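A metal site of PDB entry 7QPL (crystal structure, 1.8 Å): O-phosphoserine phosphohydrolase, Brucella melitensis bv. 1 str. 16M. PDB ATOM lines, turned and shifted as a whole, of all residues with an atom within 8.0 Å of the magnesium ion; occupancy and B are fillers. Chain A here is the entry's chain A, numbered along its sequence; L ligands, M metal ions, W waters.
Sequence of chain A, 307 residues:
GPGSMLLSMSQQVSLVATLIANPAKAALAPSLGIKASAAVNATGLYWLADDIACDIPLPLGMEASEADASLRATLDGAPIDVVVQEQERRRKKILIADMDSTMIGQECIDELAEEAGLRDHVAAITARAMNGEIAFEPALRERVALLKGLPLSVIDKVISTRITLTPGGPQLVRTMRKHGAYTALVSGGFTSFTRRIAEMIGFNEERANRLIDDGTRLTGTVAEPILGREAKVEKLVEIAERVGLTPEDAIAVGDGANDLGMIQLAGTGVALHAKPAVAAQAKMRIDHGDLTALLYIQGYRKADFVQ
The side-chain amide oxygen (OD1) of Asn 258 sits close to the side-chain carboxylate (OD1) of Asp 259 (3.3 Å).
The side-chain carboxylate of Asp 98 is in salt-bridge range of the side-chain amino group of Lys 232 (3.0 Å).
OD2 of Asp 259 is in hydrogen-bond range of N of Asp 255, at 3.0 Å.
OD2 of Asp 98 sits close to OG1 of Thr 102.
The side-chain amino group of Lys 232 lies within salt-bridge range of the side-chain carboxylate of Asp 259 (2.7 Å).
The backbone NH (N) of Asp 255 lies within hydrogen-bond range of the side-chain hydroxyl (OG1) of Thr 102 (3.2 Å).
O of Val 253 sits at hydrogen-bond distance from N of Asp 98 (2.9 Å).
OD2 of Asp 259 lies within hydrogen-bond range of N of Gly 256 (3.0 Å).
Asp 259 touches the magnesium ion.
The nearest printed residue that does not touch the magnesium ion is Thr 102 (4.1 Å).
The magnesium ion is bound by OD2 of Asp 98 (2.0 Å), O3 of the ligand (2.0 Å), water W1 (2.1 Å), water W2 (2.1 Å), OD1 of Asp 255 (2.1 Å) and O of Asp 100 (2.2 Å).
Water W2 bridges the side-chain carboxylate (OD2) of Asp 259 (2.6 Å) and the side-chain amide oxygen (OD1) of Asn 258 (3.0 Å).
Water W1 lies within hydrogen-bond range of the side-chain carboxylate of Glu 107 and the side-chain carboxylate of Asp 255.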
ATOM      1  N   ALA A  97     -11.476  -9.644  -1.447  1.00  0.00           N
ATOM      2  CA  ALA A  97     -11.868 -11.052  -1.544  1.00  0.00           C
ATOM      3  C   ALA A  97     -10.910 -11.928  -0.762  1.00  0.00           C
ATOM      4  O   ALA A  97      -9.689 -11.778  -0.851  1.00  0.00           O
ATOM      5  CB  ALA A  97     -11.885 -11.490  -3.013  1.00  0.00           C
ATOM      6  N   ASP A  98     -11.471 -12.872  -0.010  1.00  0.00           N
ATOM      7  CA  ASP A  98     -10.683 -13.851   0.720  1.00  0.00           C
ATOM      8  C   ASP A  98     -10.026 -14.855  -0.227  1.00  0.00           C
ATOM      9  O   ASP A  98     -10.578 -15.169  -1.286  1.00  0.00           O
ATOM     10  CB  ASP A  98     -11.584 -14.634   1.669  1.00  0.00           C
ATOM     11  CG  ASP A  98     -10.813 -15.649   2.428  1.00  0.00           C
ATOM     12  OD1 ASP A  98      -9.779 -15.255   2.989  1.00  0.00           O
ATOM     13  OD2 ASP A  98     -11.207 -16.830   2.447  1.00  0.00           O
ATOM     14  N   MET A  99      -8.866 -15.419   0.170  1.00  0.00           N
ATOM     15  CA  MET A  99      -8.235 -16.398  -0.730  1.00  0.00           C
ATOM     16  C   MET A  99      -8.689 -17.829  -0.456  1.00  0.00           C
ATOM     17  O   MET A  99      -9.407 -18.410  -1.278  1.00  0.00           O
ATOM     18  CB  MET A  99      -6.713 -16.259  -0.700  1.00  0.00           C
ATOM     19  CG  MET A  99      -6.072 -17.268  -1.670  1.00  0.00           C
ATOM     20  SD  MET A  99      -4.295 -17.538  -1.556  1.00  0.00           S
ATOM     21  CE  MET A  99      -4.043 -18.004   0.160  1.00  0.00           C
ATOM     22  N   ASP A 100      -8.306 -18.417   0.683  1.00  0.00           N
ATOM     23  CA  ASP A 100      -8.546 -19.850   0.880  1.00  0.00           C
ATOM     24  C   ASP A 100     -10.031 -20.189   0.932  1.00  0.00           C
ATOM     25  O   ASP A 100     -10.778 -19.613   1.724  1.00  0.00           O
ATOM     26  CB  ASP A 100      -7.894 -20.340   2.168  1.00  0.00           C
ATOM     27  CG  ASP A 100      -6.401 -20.280   2.132  1.00  0.00           C
ATOM     28  OD1 ASP A 100      -5.812 -20.874   1.225  1.00  0.00           O
ATOM     29  OD2 ASP A 100      -5.817 -19.613   3.018  1.00  0.00           O
ATOM     30  N   SER A 101     -10.423 -21.170   0.125  1.00  0.00           N
ATOM     31  CA  SER A 101     -11.788 -21.662  -0.028  1.00  0.00           C
ATOM     32  C   SER A 101     -12.729 -20.585  -0.554  1.00  0.00           C
ATOM     33  O   SER A 101     -13.950 -20.757  -0.486  1.00  0.00           O
ATOM     34  CB  SER A 101     -12.343 -22.249   1.285  1.00  0.00           C
ATOM     35  OG  SER A 101     -11.553 -23.365   1.687  1.00  0.00           O
ATOM     36  N   THR A 102     -12.191 -19.484  -1.054  1.00  0.00           N
ATOM     37  CA  THR A 102     -13.016 -18.459  -1.683  1.00  0.00           C
ATOM     38  C   THR A 102     -12.515 -18.262  -3.113  1.00  0.00           C
ATOM     39  O   THR A 102     -13.152 -18.774  -4.033  1.00  0.00           O
ATOM     40  CB  THR A 102     -13.017 -17.150  -0.873  1.00  0.00           C
ATOM     41  OG1 THR A 102     -13.694 -17.385   0.381  1.00  0.00           O
ATOM     42  CG2 THR A 102     -13.778 -16.057  -1.631  1.00  0.00           C
ATOM     43  N   MET A 103     -11.364 -17.598  -3.324  1.00  0.00           N
ATOM     44  CA  MET A 103     -10.882 -17.491  -4.694  1.00  0.00           C
ATOM     45  C   MET A 103     -10.135 -18.721  -5.179  1.00  0.00           C
ATOM     46  O   MET A 103      -9.953 -18.880  -6.386  1.00  0.00           O
ATOM     47  CB  MET A 103     -10.017 -16.226  -4.899  1.00  0.00           C
ATOM     48  CG  MET A 103     -10.706 -15.051  -4.257  1.00  0.00           C
ATOM     49  SD  MET A 103     -12.025 -14.450  -5.382  1.00  0.00           S
ATOM     50  CE  MET A 103     -11.303 -14.609  -7.031  1.00  0.00           C
ATOM     51  N   ILE A 104      -9.713 -19.608  -4.270  1.00  0.00           N
ATOM     52  CA  ILE A 104      -9.163 -20.901  -4.675  1.00  0.00           C
ATOM     53  C   ILE A 104     -10.001 -21.994  -4.030  1.00  0.00           C
ATOM     54  O   ILE A 104     -10.701 -21.761  -3.034  1.00  0.00           O
ATOM     55  CB  ILE A 104      -7.677 -21.049  -4.310  1.00  0.00           C
ATOM     56  CG1 ILE A 104      -7.500 -20.897  -2.789  1.00  0.00           C
ATOM     57  CG2 ILE A 104      -6.837 -20.044  -5.084  1.00  0.00           C
ATOM     58  CD1 ILE A 104      -6.099 -21.298  -2.299  1.00  0.00           C
ATOM     59  N   GLN A 106      -8.973 -24.571  -2.355  1.00  0.00           N
ATOM     60  CA  GLN A 106      -8.299 -25.271  -1.286  1.00  0.00           C
ATOM     61  C   GLN A 106      -8.016 -24.357  -0.101  1.00  0.00           C
ATOM     62  O   GLN A 106      -8.224 -23.134  -0.160  1.00  0.00           O
ATOM     63  CB  GLN A 106      -6.960 -25.865  -1.784  1.00  0.00           C
ATOM     64  CG  GLN A 106      -7.114 -26.931  -2.875  1.00  0.00           C
ATOM     65  CD  GLN A 106      -7.499 -26.340  -4.222  1.00  0.00           C
ATOM     66  OE1 GLN A 106      -7.092 -25.223  -4.558  1.00  0.00           O
ATOM     67  NE2 GLN A 106      -8.305 -27.062  -4.978  1.00  0.00           N
ATOM     68  N   GLU A 107      -7.524 -24.961   0.975  1.00  0.00           N
ATOM     69  CA  GLU A 107      -6.929 -24.264   2.117  1.00  0.00           C
ATOM     70  C   GLU A 107      -5.422 -24.458   2.006  1.00  0.00           C
ATOM     71  O   GLU A 107      -4.937 -25.588   2.124  1.00  0.00           O
ATOM     72  CB  GLU A 107      -7.464 -24.827   3.427  1.00  0.00           C
ATOM     73  CG  GLU A 107      -8.965 -24.563   3.657  1.00  0.00           C
ATOM     74  CD  GLU A 107      -9.195 -23.130   4.072  1.00  0.00           C
ATOM     75  OE1 GLU A 107      -8.309 -22.570   4.757  1.00  0.00           O
ATOM     76  OE2 GLU A 107     -10.239 -22.565   3.709  1.00  0.00           O
ATOM     77  N   THR A 126      -8.406 -26.441  10.859  1.00  0.00           N
ATOM     78  CA  THR A 126      -8.830 -25.441   9.891  1.00  0.00           C
ATOM     79  C   THR A 126     -10.347 -25.335   9.819  1.00  0.00           C
ATOM     80  O   THR A 126     -10.894 -24.233   9.794  1.00  0.00           O
ATOM     81  CB  THR A 126      -8.269 -25.796   8.512  1.00  0.00           C
ATOM     82  OG1 THR A 126      -6.835 -25.806   8.592  1.00  0.00           O
ATOM     83  CG2 THR A 126      -8.701 -24.776   7.465  1.00  0.00           C
ATOM     84  N   MET A 130     -12.485 -22.049  10.449  1.00  0.00           N
ATOM     85  CA  MET A 130     -13.400 -21.536   9.441  1.00  0.00           C
ATOM     86  C   MET A 130     -14.793 -21.313  10.017  1.00  0.00           C
ATOM     87  O   MET A 130     -15.487 -20.342   9.660  1.00  0.00           O
ATOM     88  CB  MET A 130     -13.474 -22.506   8.264  1.00  0.00           C
ATOM     89  CG  MET A 130     -12.196 -22.632   7.457  1.00  0.00           C
ATOM     90  SD  MET A 130     -12.123 -24.137   6.451  1.00  0.00           S
ATOM     91  CE  MET A 130     -13.802 -24.193   5.846  1.00  0.00           C
ATOM     92  N   PHE A 136      -8.984 -17.436  15.297  1.00  0.00           N
ATOM     93  CA  PHE A 136      -8.114 -17.641  14.142  1.00  0.00           C
ATOM     94  C   PHE A 136      -6.646 -17.692  14.532  1.00  0.00           C
ATOM     95  O   PHE A 136      -5.902 -18.555  14.061  1.00  0.00           O
ATOM     96  CB  PHE A 136      -8.329 -16.553  13.105  1.00  0.00           C
ATOM     97  CG  PHE A 136      -7.469 -16.735  11.918  1.00  0.00           C
ATOM     98  CD1 PHE A 136      -7.758 -17.716  10.979  1.00  0.00           C
ATOM     99  CD2 PHE A 136      -6.302 -15.984  11.789  1.00  0.00           C
ATOM    100  CE1 PHE A 136      -6.939 -17.910   9.900  1.00  0.00           C
ATOM    101  CE2 PHE A 136      -5.483 -16.182  10.720  1.00  0.00           C
ATOM    102  CZ  PHE A 136      -5.794 -17.149   9.767  1.00  0.00           C
ATOM    103  N   VAL A 186      -7.184 -10.791   0.107  1.00  0.00           N
ATOM    104  CA  VAL A 186      -6.690 -10.810   1.484  1.00  0.00           C
ATOM    105  C   VAL A 186      -6.810 -12.236   2.025  1.00  0.00           C
ATOM    106  O   VAL A 186      -7.617 -13.040   1.551  1.00  0.00           O
ATOM    107  CB  VAL A 186      -7.419  -9.810   2.403  1.00  0.00           C
ATOM    108  CG1 VAL A 186      -7.202  -8.386   1.918  1.00  0.00           C
ATOM    109  CG2 VAL A 186      -8.928 -10.159   2.508  1.00  0.00           C
ATOM    110  N   SER A 187      -5.971 -12.555   2.997  1.00  0.00           N
ATOM    111  CA  SER A 187      -5.936 -13.928   3.480  1.00  0.00           C
ATOM    112  C   SER A 187      -5.269 -14.002   4.847  1.00  0.00           C
ATOM    113  O   SER A 187      -4.291 -13.293   5.094  1.00  0.00           O
ATOM    114  CB  SER A 187      -5.173 -14.837   2.500  1.00  0.00           C
ATOM    115  OG  SER A 187      -5.287 -16.189   2.898  1.00  0.00           O
ATOM    116  N   GLY A 188      -5.819 -14.840   5.724  1.00  0.00           N
ATOM    117  CA  GLY A 188      -5.064 -15.339   6.865  1.00  0.00           C
ATOM    118  C   GLY A 188      -4.039 -16.394   6.498  1.00  0.00           C
ATOM    119  O   GLY A 188      -3.254 -16.809   7.355  1.00  0.00           O
ATOM    120  N   GLY A 189      -4.046 -16.828   5.240  1.00  0.00           N
ATOM    121  CA  GLY A 189      -3.013 -17.686   4.664  1.00  0.00           C
ATOM    122  C   GLY A 189      -1.729 -16.929   4.393  1.00  0.00           C
ATOM    123  O   GLY A 189      -1.453 -15.953   5.088  1.00  0.00           O
ATOM    124  N   LYS A 232      -8.453  -7.949   8.078  1.00  0.00           N
ATOM    125  CA  LYS A 232      -9.198  -7.822   6.832  1.00  0.00           C
ATOM    126  C   LYS A 232     -10.074  -6.579   6.861  1.00  0.00           C
ATOM    127  O   LYS A 232     -10.203  -5.881   5.846  1.00  0.00           O
ATOM    128  CB  LYS A 232     -10.037  -9.092   6.557  1.00  0.00           C
ATOM    129  CG  LYS A 232      -9.166 -10.335   6.373  1.00  0.00           C
ATOM    130  CD  LYS A 232     -10.011 -11.603   6.111  1.00  0.00           C
ATOM    131  CE  LYS A 232      -9.103 -12.756   5.733  1.00  0.00           C
ATOM    132  NZ  LYS A 232      -9.798 -14.114   5.789  1.00  0.00           N
ATOM    133  N   VAL A 253     -16.062 -10.458  -0.147  1.00  0.00           N
ATOM    134  CA  VAL A 253     -16.538 -11.839  -0.289  1.00  0.00           C
ATOM    135  C   VAL A 253     -15.601 -12.756   0.465  1.00  0.00           C
ATOM    136  O   VAL A 253     -14.371 -12.620   0.391  1.00  0.00           O
ATOM    137  CB  VAL A 253     -16.669 -12.261  -1.762  1.00  0.00           C
ATOM    138  CG1 VAL A 253     -15.296 -12.164  -2.476  1.00  0.00           C
ATOM    139  CG2 VAL A 253     -17.324 -13.702  -1.880  1.00  0.00           C
ATOM    140  N   GLY A 254     -16.177 -13.697   1.209  1.00  0.00           N
ATOM    141  CA  GLY A 254     -15.367 -14.718   1.829  1.00  0.00           C
ATOM    142  C   GLY A 254     -16.248 -15.871   2.263  1.00  0.00           C
ATOM    143  O   GLY A 254     -17.466 -15.869   2.036  1.00  0.00           O
ATOM    144  N   ASP A 255     -15.610 -16.859   2.873  1.00  0.00           N
ATOM    145  CA  ASP A 255     -16.274 -18.115   3.216  1.00  0.00           C
ATOM    146  C   ASP A 255     -16.253 -18.426   4.706  1.00  0.00           C
ATOM    147  O   ASP A 255     -16.954 -19.376   5.127  1.00  0.00           O
ATOM    148  CB  ASP A 255     -15.591 -19.282   2.490  1.00  0.00           C
ATOM    149  CG  ASP A 255     -14.208 -19.596   3.077  1.00  0.00           C
ATOM    150  OD1 ASP A 255     -13.300 -18.737   2.980  1.00  0.00           O
ATOM    151  OD2 ASP A 255     -14.035 -20.679   3.679  1.00  0.00           O
ATOM    152  N   GLY A 256     -15.451 -17.715   5.502  1.00  0.00           N
ATOM    153  CA  GLY A 256     -15.103 -18.158   6.832  1.00  0.00           C
ATOM    154  C   GLY A 256     -15.454 -17.125   7.894  1.00  0.00           C
ATOM    155  O   GLY A 256     -15.743 -15.953   7.587  1.00  0.00           O
ATOM    156  N   ALA A 257     -15.431 -17.578   9.153  1.00  0.00           N
ATOM    157  CA  ALA A 257     -15.728 -16.679  10.269  1.00  0.00           C
ATOM    158  C   ALA A 257     -14.809 -15.463  10.257  1.00  0.00           C
ATOM    159  O   ALA A 257     -15.247 -14.336  10.553  1.00  0.00           O
ATOM    160  CB  ALA A 257     -15.614 -17.426  11.594  1.00  0.00           C
ATOM    161  N   ASN A 258     -13.536 -15.666   9.890  1.00  0.00           N
ATOM    162  CA  ASN A 258     -12.581 -14.555   9.904  1.00  0.00           C
ATOM    163  C   ASN A 258     -12.842 -13.551   8.778  1.00  0.00           C
ATOM    164  O   ASN A 258     -12.172 -12.514   8.742  1.00  0.00           O
ATOM    165  CB  ASN A 258     -11.131 -15.073   9.872  1.00  0.00           C
ATOM    166  CG  ASN A 258     -10.688 -15.605   8.500  1.00  0.00           C
ATOM    167  OD1 ASN A 258     -11.445 -15.647   7.520  1.00  0.00           O
ATOM    168  ND2 ASN A 258      -9.409 -16.019   8.423  1.00  0.00           N
ATOM    169  N   ASP A 259     -13.794 -13.820   7.879  1.00  0.00           N
ATOM    170  CA  ASP A 259     -14.172 -12.838   6.866  1.00  0.00           C
ATOM    171  C   ASP A 259     -15.334 -11.966   7.273  1.00  0.00           C
ATOM    172  O   ASP A 259     -15.636 -10.997   6.577  1.00  0.00           O
ATOM    173  CB  ASP A 259     -14.548 -13.523   5.552  1.00  0.00           C
ATOM    174  CG  ASP A 259     -13.430 -14.325   4.993  1.00  0.00           C
ATOM    175  OD1 ASP A 259     -12.329 -13.745   4.914  1.00  0.00           O
ATOM    176  OD2 ASP A 259     -13.617 -15.522   4.662  1.00  0.00           O
ATOM    177  N   MET A 262     -14.967  -7.907   7.460  1.00  0.00           N
ATOM    178  CA  MET A 262     -15.012  -7.154   6.208  1.00  0.00           C
ATOM    179  C   MET A 262     -16.337  -7.342   5.495  1.00  0.00           C
ATOM    180  O   MET A 262     -16.839  -6.401   4.873  1.00  0.00           O
ATOM    181  CB  MET A 262     -13.842  -7.550   5.310  1.00  0.00           C
ATOM    182  CG  MET A 262     -13.921  -8.934   4.695  1.00  0.00           C
ATOM    183  SD  MET A 262     -12.523  -9.168   3.550  1.00  0.00           S
ATOM    184  CE  MET A 262     -12.937 -10.791   2.871  1.00  0.00           C
ATOM    185  N   LEU A 272     -19.780 -16.692   0.559  1.00  0.00           N
ATOM    186  CA  LEU A 272     -19.773 -17.568  -0.617  1.00  0.00           C
ATOM    187  C   LEU A 272     -19.574 -19.016  -0.185  1.00  0.00           C
ATOM    188  O   LEU A 272     -18.495 -19.368   0.306  1.00  0.00           O
ATOM    189  CB  LEU A 272     -18.663 -17.140  -1.583  1.00  0.00           C
ATOM    190  CG  LEU A 272     -18.516 -17.995  -2.852  1.00  0.00           C
ATOM    191  CD1 LEU A 272     -19.716 -17.762  -3.782  1.00  0.00           C
ATOM    192  CD2 LEU A 272     -17.194 -17.725  -3.570  1.00  0.00           C
HETATM  193  P1  LIG L   1      -8.164 -17.477   4.501  1.00  0.00           P
HETATM  194  O1  LIG L   1      -6.969 -18.310   4.892  1.00  0.00           O
HETATM  195  O2  LIG L   1      -8.312 -16.381   5.549  1.00  0.00           O
HETATM  196  O3  LIG L   1      -9.450 -18.298   4.422  1.00  0.00           O
HETATM  197  O4  LIG L   1      -7.833 -16.831   3.173  1.00  0.00           O
HETATM  198 MG    MG M   1     -11.283 -18.531   3.554  1.00  0.00          MG
HETATM  199  O   HOH W   1     -11.433 -20.316   4.573  1.00  0.00           O
HETATM  200  O   HOH W   2     -11.944 -17.436   5.216  1.00  0.00           O
